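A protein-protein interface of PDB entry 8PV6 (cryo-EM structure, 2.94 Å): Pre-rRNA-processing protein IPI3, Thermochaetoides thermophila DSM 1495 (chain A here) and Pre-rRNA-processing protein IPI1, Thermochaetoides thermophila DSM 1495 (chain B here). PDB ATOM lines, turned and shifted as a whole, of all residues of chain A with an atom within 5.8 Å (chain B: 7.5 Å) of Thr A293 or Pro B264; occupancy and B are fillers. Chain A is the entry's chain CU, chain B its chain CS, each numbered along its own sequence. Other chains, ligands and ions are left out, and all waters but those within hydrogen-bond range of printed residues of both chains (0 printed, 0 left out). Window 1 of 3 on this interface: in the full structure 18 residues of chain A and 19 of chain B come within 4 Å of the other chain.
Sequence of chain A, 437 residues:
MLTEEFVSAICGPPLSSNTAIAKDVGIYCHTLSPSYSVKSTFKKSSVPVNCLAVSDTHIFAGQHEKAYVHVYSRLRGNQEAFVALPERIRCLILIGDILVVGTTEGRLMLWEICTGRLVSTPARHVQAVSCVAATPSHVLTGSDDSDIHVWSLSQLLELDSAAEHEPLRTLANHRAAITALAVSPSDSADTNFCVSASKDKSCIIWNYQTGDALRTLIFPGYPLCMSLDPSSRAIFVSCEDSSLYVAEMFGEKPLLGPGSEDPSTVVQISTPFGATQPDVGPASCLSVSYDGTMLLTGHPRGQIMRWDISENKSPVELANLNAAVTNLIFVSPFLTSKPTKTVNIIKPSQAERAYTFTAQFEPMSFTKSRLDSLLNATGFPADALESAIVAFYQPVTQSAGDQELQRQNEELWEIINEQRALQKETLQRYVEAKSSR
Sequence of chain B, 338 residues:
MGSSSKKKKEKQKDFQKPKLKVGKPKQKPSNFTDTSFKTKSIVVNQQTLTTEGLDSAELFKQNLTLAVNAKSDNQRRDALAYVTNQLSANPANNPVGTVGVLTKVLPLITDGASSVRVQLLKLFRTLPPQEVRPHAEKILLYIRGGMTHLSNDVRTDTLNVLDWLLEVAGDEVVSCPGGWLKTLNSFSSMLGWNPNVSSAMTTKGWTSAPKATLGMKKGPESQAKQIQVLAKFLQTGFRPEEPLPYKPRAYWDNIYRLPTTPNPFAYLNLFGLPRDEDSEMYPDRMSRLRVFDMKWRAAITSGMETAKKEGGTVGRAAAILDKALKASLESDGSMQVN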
ATOM      1  N   VAL A 288      21.169  30.567 -11.657  1.00  0.00           N
ATOM      2  CA  VAL A 288      20.855  29.817 -10.445  1.00  0.00           C
ATOM      3  C   VAL A 288      21.912  28.737 -10.265  1.00  0.00           C
ATOM      4  O   VAL A 288      22.351  28.122 -11.243  1.00  0.00           O
ATOM      5  CB  VAL A 288      19.439  29.203 -10.517  1.00  0.00           C
ATOM      6  CG1 VAL A 288      19.060  28.538  -9.210  1.00  0.00           C
ATOM      7  CG2 VAL A 288      18.420  30.267 -10.867  1.00  0.00           C
ATOM      8  N   SER A 289      22.329  28.511  -9.018  1.00  0.00           N
ATOM      9  CA  SER A 289      23.390  27.558  -8.734  1.00  0.00           C
ATOM     10  C   SER A 289      22.935  26.119  -8.977  1.00  0.00           C
ATOM     11  O   SER A 289      21.763  25.841  -9.252  1.00  0.00           O
ATOM     12  CB  SER A 289      23.867  27.709  -7.291  1.00  0.00           C
ATOM     13  OG  SER A 289      22.774  27.704  -6.393  1.00  0.00           O
ATOM     14  N   ASP A 291      22.880  23.690  -6.739  1.00  0.00           N
ATOM     15  CA  ASP A 291      21.962  23.327  -5.667  1.00  0.00           C
ATOM     16  C   ASP A 291      20.600  23.976  -5.873  1.00  0.00           C
ATOM     17  O   ASP A 291      19.564  23.376  -5.569  1.00  0.00           O
ATOM     18  CB  ASP A 291      22.554  23.738  -4.319  1.00  0.00           C
ATOM     19  CG  ASP A 291      21.969  22.957  -3.163  1.00  0.00           C
ATOM     20  OD1 ASP A 291      22.494  23.082  -2.038  1.00  0.00           O
ATOM     21  OD2 ASP A 291      20.998  22.205  -3.380  1.00  0.00           O
ATOM     22  N   GLY A 292      20.583  25.197  -6.400  1.00  0.00           N
ATOM     23  CA  GLY A 292      19.366  25.959  -6.557  1.00  0.00           C
ATOM     24  C   GLY A 292      19.085  26.931  -5.435  1.00  0.00           C
ATOM     25  O   GLY A 292      18.064  27.627  -5.482  1.00  0.00           O
ATOM     26  N   THR A 293      19.959  26.997  -4.428  1.00  0.00           N
ATOM     27  CA  THR A 293      19.718  27.885  -3.298  1.00  0.00           C
ATOM     28  C   THR A 293      20.353  29.252  -3.519  1.00  0.00           C
ATOM     29  O   THR A 293      19.838  30.268  -3.038  1.00  0.00           O
ATOM     30  CB  THR A 293      20.249  27.251  -2.016  1.00  0.00           C
ATOM     31  OG1 THR A 293      21.681  27.243  -2.046  1.00  0.00           O
ATOM     32  CG2 THR A 293      19.753  25.823  -1.897  1.00  0.00           C
ATOM     33  N   MET A 294      21.468  29.300  -4.241  1.00  0.00           N
ATOM     34  CA  MET A 294      22.167  30.547  -4.521  1.00  0.00           C
ATOM     35  C   MET A 294      21.796  31.043  -5.910  1.00  0.00           C
ATOM     36  O   MET A 294      21.512  30.250  -6.814  1.00  0.00           O
ATOM     37  CB  MET A 294      23.687  30.387  -4.412  1.00  0.00           C
ATOM     38  CG  MET A 294      24.165  29.828  -3.085  1.00  0.00           C
ATOM     39  SD  MET A 294      25.847  29.188  -3.167  1.00  0.00           S
ATOM     40  CE  MET A 294      25.667  27.640  -2.285  1.00  0.00           C
ATOM     41  N   LEU A 295      21.821  32.361  -6.071  1.00  0.00           N
ATOM     42  CA  LEU A 295      21.340  33.023  -7.272  1.00  0.00           C
ATOM     43  C   LEU A 295      22.245  34.210  -7.565  1.00  0.00           C
ATOM     44  O   LEU A 295      22.373  35.115  -6.736  1.00  0.00           O
ATOM     45  CB  LEU A 295      19.887  33.461  -7.077  1.00  0.00           C
ATOM     46  CG  LEU A 295      19.010  33.852  -8.257  1.00  0.00           C
ATOM     47  CD1 LEU A 295      17.586  33.440  -7.971  1.00  0.00           C
ATOM     48  CD2 LEU A 295      19.075  35.338  -8.473  1.00  0.00           C
ATOM     49  N   TRP A 307      22.290  36.011  -4.226  1.00  0.00           N
ATOM     50  CA  TRP A 307      21.024  35.988  -3.512  1.00  0.00           C
ATOM     51  C   TRP A 307      20.829  34.617  -2.882  1.00  0.00           C
ATOM     52  O   TRP A 307      20.645  33.624  -3.593  1.00  0.00           O
ATOM     53  CB  TRP A 307      19.848  36.302  -4.442  1.00  0.00           C
ATOM     54  CG  TRP A 307      19.979  37.558  -5.263  1.00  0.00           C
ATOM     55  CD1 TRP A 307      20.835  37.781  -6.301  1.00  0.00           C
ATOM     56  CD2 TRP A 307      19.201  38.753  -5.125  1.00  0.00           C
ATOM     57  NE1 TRP A 307      20.650  39.042  -6.806  1.00  0.00           N
ATOM     58  CE2 TRP A 307      19.650  39.659  -6.104  1.00  0.00           C
ATOM     59  CE3 TRP A 307      18.171  39.146  -4.266  1.00  0.00           C
ATOM     60  CZ2 TRP A 307      19.109  40.932  -6.246  1.00  0.00           C
ATOM     61  CZ3 TRP A 307      17.633  40.411  -4.409  1.00  0.00           C
ATOM     62  CH2 TRP A 307      18.104  41.288  -5.392  1.00  0.00           C
ATOM     63  N   ASP A 308      20.866  34.565  -1.555  1.00  0.00           N
ATOM     64  CA  ASP A 308      20.533  33.359  -0.811  1.00  0.00           C
ATOM     65  C   ASP A 308      19.030  33.358  -0.573  1.00  0.00           C
ATOM     66  O   ASP A 308      18.540  34.080   0.301  1.00  0.00           O
ATOM     67  CB  ASP A 308      21.296  33.300   0.513  1.00  0.00           C
ATOM     68  CG  ASP A 308      22.798  33.294   0.318  1.00  0.00           C
ATOM     69  OD1 ASP A 308      23.247  33.289  -0.846  1.00  0.00           O
ATOM     70  OD2 ASP A 308      23.530  33.293   1.330  1.00  0.00           O
ATOM     71  N   ILE A 309      18.309  32.545  -1.353  1.00  0.00           N
ATOM     72  CA  ILE A 309      16.848  32.608  -1.387  1.00  0.00           C
ATOM     73  C   ILE A 309      16.251  32.239  -0.035  1.00  0.00           C
ATOM     74  O   ILE A 309      15.314  32.889   0.446  1.00  0.00           O
ATOM     75  CB  ILE A 309      16.310  31.704  -2.509  1.00  0.00           C
ATOM     76  CG1 ILE A 309      17.061  31.970  -3.811  1.00  0.00           C
ATOM     77  CG2 ILE A 309      14.819  31.914  -2.700  1.00  0.00           C
ATOM     78  CD1 ILE A 309      16.847  30.907  -4.858  1.00  0.00           C
ATOM     79  N   SER A 310      16.779  31.196   0.599  1.00  0.00           N
ATOM     80  CA  SER A 310      16.286  30.771   1.901  1.00  0.00           C
ATOM     81  C   SER A 310      16.703  31.737   3.005  1.00  0.00           C
ATOM     82  O   SER A 310      15.927  32.006   3.926  1.00  0.00           O
ATOM     83  CB  SER A 310      16.783  29.360   2.219  1.00  0.00           C
ATOM     84  N   LEU B 258       9.818  25.011  -3.283  1.00  0.00           N
ATOM     85  CA  LEU B 258      11.178  25.344  -2.896  1.00  0.00           C
ATOM     86  C   LEU B 258      11.387  25.095  -1.402  1.00  0.00           C
ATOM     87  O   LEU B 258      10.439  25.171  -0.616  1.00  0.00           O
ATOM     88  CB  LEU B 258      11.484  26.802  -3.223  1.00  0.00           C
ATOM     89  CG  LEU B 258      11.614  27.179  -4.698  1.00  0.00           C
ATOM     90  CD1 LEU B 258      11.816  28.675  -4.823  1.00  0.00           C
ATOM     91  CD2 LEU B 258      12.759  26.430  -5.347  1.00  0.00           C
ATOM     92  N   PRO B 259      12.614  24.775  -0.990  1.00  0.00           N
ATOM     93  CA  PRO B 259      12.879  24.576   0.440  1.00  0.00           C
ATOM     94  C   PRO B 259      12.765  25.882   1.214  1.00  0.00           C
ATOM     95  O   PRO B 259      13.448  26.863   0.915  1.00  0.00           O
ATOM     96  CB  PRO B 259      14.312  24.032   0.460  1.00  0.00           C
ATOM     97  CG  PRO B 259      14.519  23.461  -0.902  1.00  0.00           C
ATOM     98  CD  PRO B 259      13.760  24.368  -1.817  1.00  0.00           C
ATOM     99  N   THR B 260      11.889  25.884   2.215  1.00  0.00           N
ATOM    100  CA  THR B 260      11.656  27.054   3.049  1.00  0.00           C
ATOM    101  C   THR B 260      12.556  27.095   4.277  1.00  0.00           C
ATOM    102  O   THR B 260      12.583  28.113   4.973  1.00  0.00           O
ATOM    103  CB  THR B 260      10.191  27.104   3.490  1.00  0.00           C
ATOM    104  OG1 THR B 260       9.914  25.999   4.359  1.00  0.00           O
ATOM    105  CG2 THR B 260       9.272  27.030   2.282  1.00  0.00           C
ATOM    106  N   THR B 261      13.286  26.020   4.557  1.00  0.00           N
ATOM    107  CA  THR B 261      14.194  26.002   5.695  1.00  0.00           C
ATOM    108  C   THR B 261      15.432  26.841   5.394  1.00  0.00           C
ATOM    109  O   THR B 261      16.041  26.685   4.332  1.00  0.00           O
ATOM    110  CB  THR B 261      14.620  24.576   6.029  1.00  0.00           C
ATOM    111  OG1 THR B 261      15.472  24.075   4.993  1.00  0.00           O
ATOM    112  CG2 THR B 261      13.401  23.675   6.158  1.00  0.00           C
ATOM    113  N   PRO B 262      15.797  27.748   6.300  1.00  0.00           N
ATOM    114  CA  PRO B 262      16.998  28.562   6.087  1.00  0.00           C
ATOM    115  C   PRO B 262      18.255  27.711   6.072  1.00  0.00           C
ATOM    116  O   PRO B 262      18.447  26.832   6.917  1.00  0.00           O
ATOM    117  CB  PRO B 262      16.991  29.526   7.279  1.00  0.00           C
ATOM    118  CG  PRO B 262      16.170  28.838   8.318  1.00  0.00           C
ATOM    119  CD  PRO B 262      15.117  28.085   7.562  1.00  0.00           C
ATOM    120  N   ASN B 263      19.119  28.011   5.099  1.00  0.00           N
ATOM    121  CA  ASN B 263      20.310  27.227   4.793  1.00  0.00           C
ATOM    122  C   ASN B 263      19.994  25.737   4.620  1.00  0.00           C
ATOM    123  O   ASN B 263      20.314  24.924   5.490  1.00  0.00           O
ATOM    124  CB  ASN B 263      21.386  27.425   5.853  1.00  0.00           C
ATOM    125  CG  ASN B 263      22.721  26.812   5.460  1.00  0.00           C
ATOM    126  OD1 ASN B 263      22.960  26.502   4.293  1.00  0.00           O
ATOM    127  ND2 ASN B 263      23.598  26.633   6.441  1.00  0.00           N
ATOM    128  N   PRO B 264      19.343  25.352   3.524  1.00  0.00           N
ATOM    129  CA  PRO B 264      19.094  23.930   3.288  1.00  0.00           C
ATOM    130  C   PRO B 264      20.354  23.236   2.804  1.00  0.00           C
ATOM    131  O   PRO B 264      21.322  23.872   2.382  1.00  0.00           O
ATOM    132  CB  PRO B 264      18.010  23.937   2.210  1.00  0.00           C
ATOM    133  CG  PRO B 264      18.303  25.155   1.430  1.00  0.00           C
ATOM    134  CD  PRO B 264      18.875  26.174   2.393  1.00  0.00           C
ATOM    135  N   PHE B 265      20.330  21.905   2.901  1.00  0.00           N
ATOM    136  CA  PHE B 265      21.411  21.011   2.489  1.00  0.00           C
ATOM    137  C   PHE B 265      22.719  21.287   3.218  1.00  0.00           C
ATOM    138  O   PHE B 265      23.795  20.987   2.692  1.00  0.00           O
ATOM    139  CB  PHE B 265      21.635  21.061   0.974  1.00  0.00           C
ATOM    140  CG  PHE B 265      20.373  20.940   0.179  1.00  0.00           C
ATOM    141  CD1 PHE B 265      19.725  19.725   0.068  1.00  0.00           C
ATOM    142  CD2 PHE B 265      19.825  22.045  -0.447  1.00  0.00           C
ATOM    143  CE1 PHE B 265      18.562  19.613  -0.655  1.00  0.00           C
ATOM    144  CE2 PHE B 265      18.660  21.936  -1.176  1.00  0.00           C
ATOM    145  CZ  PHE B 265      18.028  20.718  -1.278  1.00  0.00           C
ATOM    146  N   ALA B 266      22.655  21.859   4.421  1.00  0.00           N
ATOM    147  CA  ALA B 266      23.864  22.045   5.213  1.00  0.00           C
ATOM    148  C   ALA B 266      24.335  20.734   5.823  1.00  0.00           C
ATOM    149  O   ALA B 266      25.521  20.583   6.130  1.00  0.00           O
ATOM    150  CB  ALA B 266      23.625  23.085   6.307  1.00  0.00           C
ATOM    151  N   TYR B 267      23.421  19.779   6.010  1.00  0.00           N
ATOM    152  CA  TYR B 267      23.801  18.477   6.541  1.00  0.00           C
ATOM    153  C   TYR B 267      24.548  17.636   5.518  1.00  0.00           C
ATOM    154  O   TYR B 267      25.271  16.710   5.904  1.00  0.00           O
ATOM    155  CB  TYR B 267      22.565  17.723   7.045  1.00  0.00           C
ATOM    156  CG  TYR B 267      21.448  17.550   6.033  1.00  0.00           C
ATOM    157  CD1 TYR B 267      20.496  18.544   5.841  1.00  0.00           C
ATOM    158  CD2 TYR B 267      21.338  16.387   5.283  1.00  0.00           C
ATOM    159  CE1 TYR B 267      19.475  18.388   4.925  1.00  0.00           C
ATOM    160  CE2 TYR B 267      20.318  16.223   4.364  1.00  0.00           C
ATOM    161  CZ  TYR B 267      19.393  17.227   4.189  1.00  0.00           C
ATOM    162  OH  TYR B 267      18.377  17.068   3.276  1.00  0.00           O
ATOM    163  N   LEU B 268      24.389  17.928   4.228  1.00  0.00           N
ATOM    164  CA  LEU B 268      25.116  17.189   3.203  1.00  0.00           C
ATOM    165  C   LEU B 268      26.598  17.537   3.201  1.00  0.00           C
ATOM    166  O   LEU B 268      27.439  16.647   3.025  1.00  0.00           O
ATOM    167  CB  LEU B 268      24.507  17.458   1.830  1.00  0.00           C
ATOM    168  CG  LEU B 268      23.041  17.064   1.691  1.00  0.00           C
ATOM    169  CD1 LEU B 268      22.521  17.405   0.311  1.00  0.00           C
ATOM    170  CD2 LEU B 268      22.902  15.589   1.962  1.00  0.00           C
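Of chain B, only Pro B264 comes within 4 Å of Thr A293. Of chain A, only Thr A293 (3.7 Å) and Ser A310 (3.8 Å) come within 4 Å of Pro B264. No residue of chain B comes within 4 Å of Gly A292. Of the printed residues of chain A, Phe B265 touches Asp A291. Printed residues of chain B within 4 Å of Ser A310: Thr B261, Pro B262, Asn B263 and Pro B264. Ala B266 touches none of the printed residues of chain A. The nearest residue of chain B that does not touch Thr A293 is Phe B265 (4.05 Å). The nearest printed residue of chain A that does not touch Pro B262 is Ile A309 (7.2 Å).
Printed residues of chain B that touch a printed residue of chain A: Thr B261, Pro B262, Asn B263, Pro B264 and Phe B265. Hydrophobic or aromatic side chains of chain B within 4 Å of the printed part of chain A: Pro B264 and Phe B265. Printed residues of chain A that touch a printed residue of chain B: Asp A291, Thr A293 and Ser A310.
Among the printed residues, merely in contact across the chains: Asp A291 with Phe B265 (3.2 Å), Ser A310 with Thr B261 (3.5 Å), Thr A293 with Pro B264 (3.7 Å), Ser A310 with Pro B264 (3.8 Å), Ser A310 with Asn B263 (3.9 Å) and Ser A310 with Pro B262 (3.96 Å).
O of Thr A293 lies within hydrogen-bond range of N of Ile A309, 3.2 Å away.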
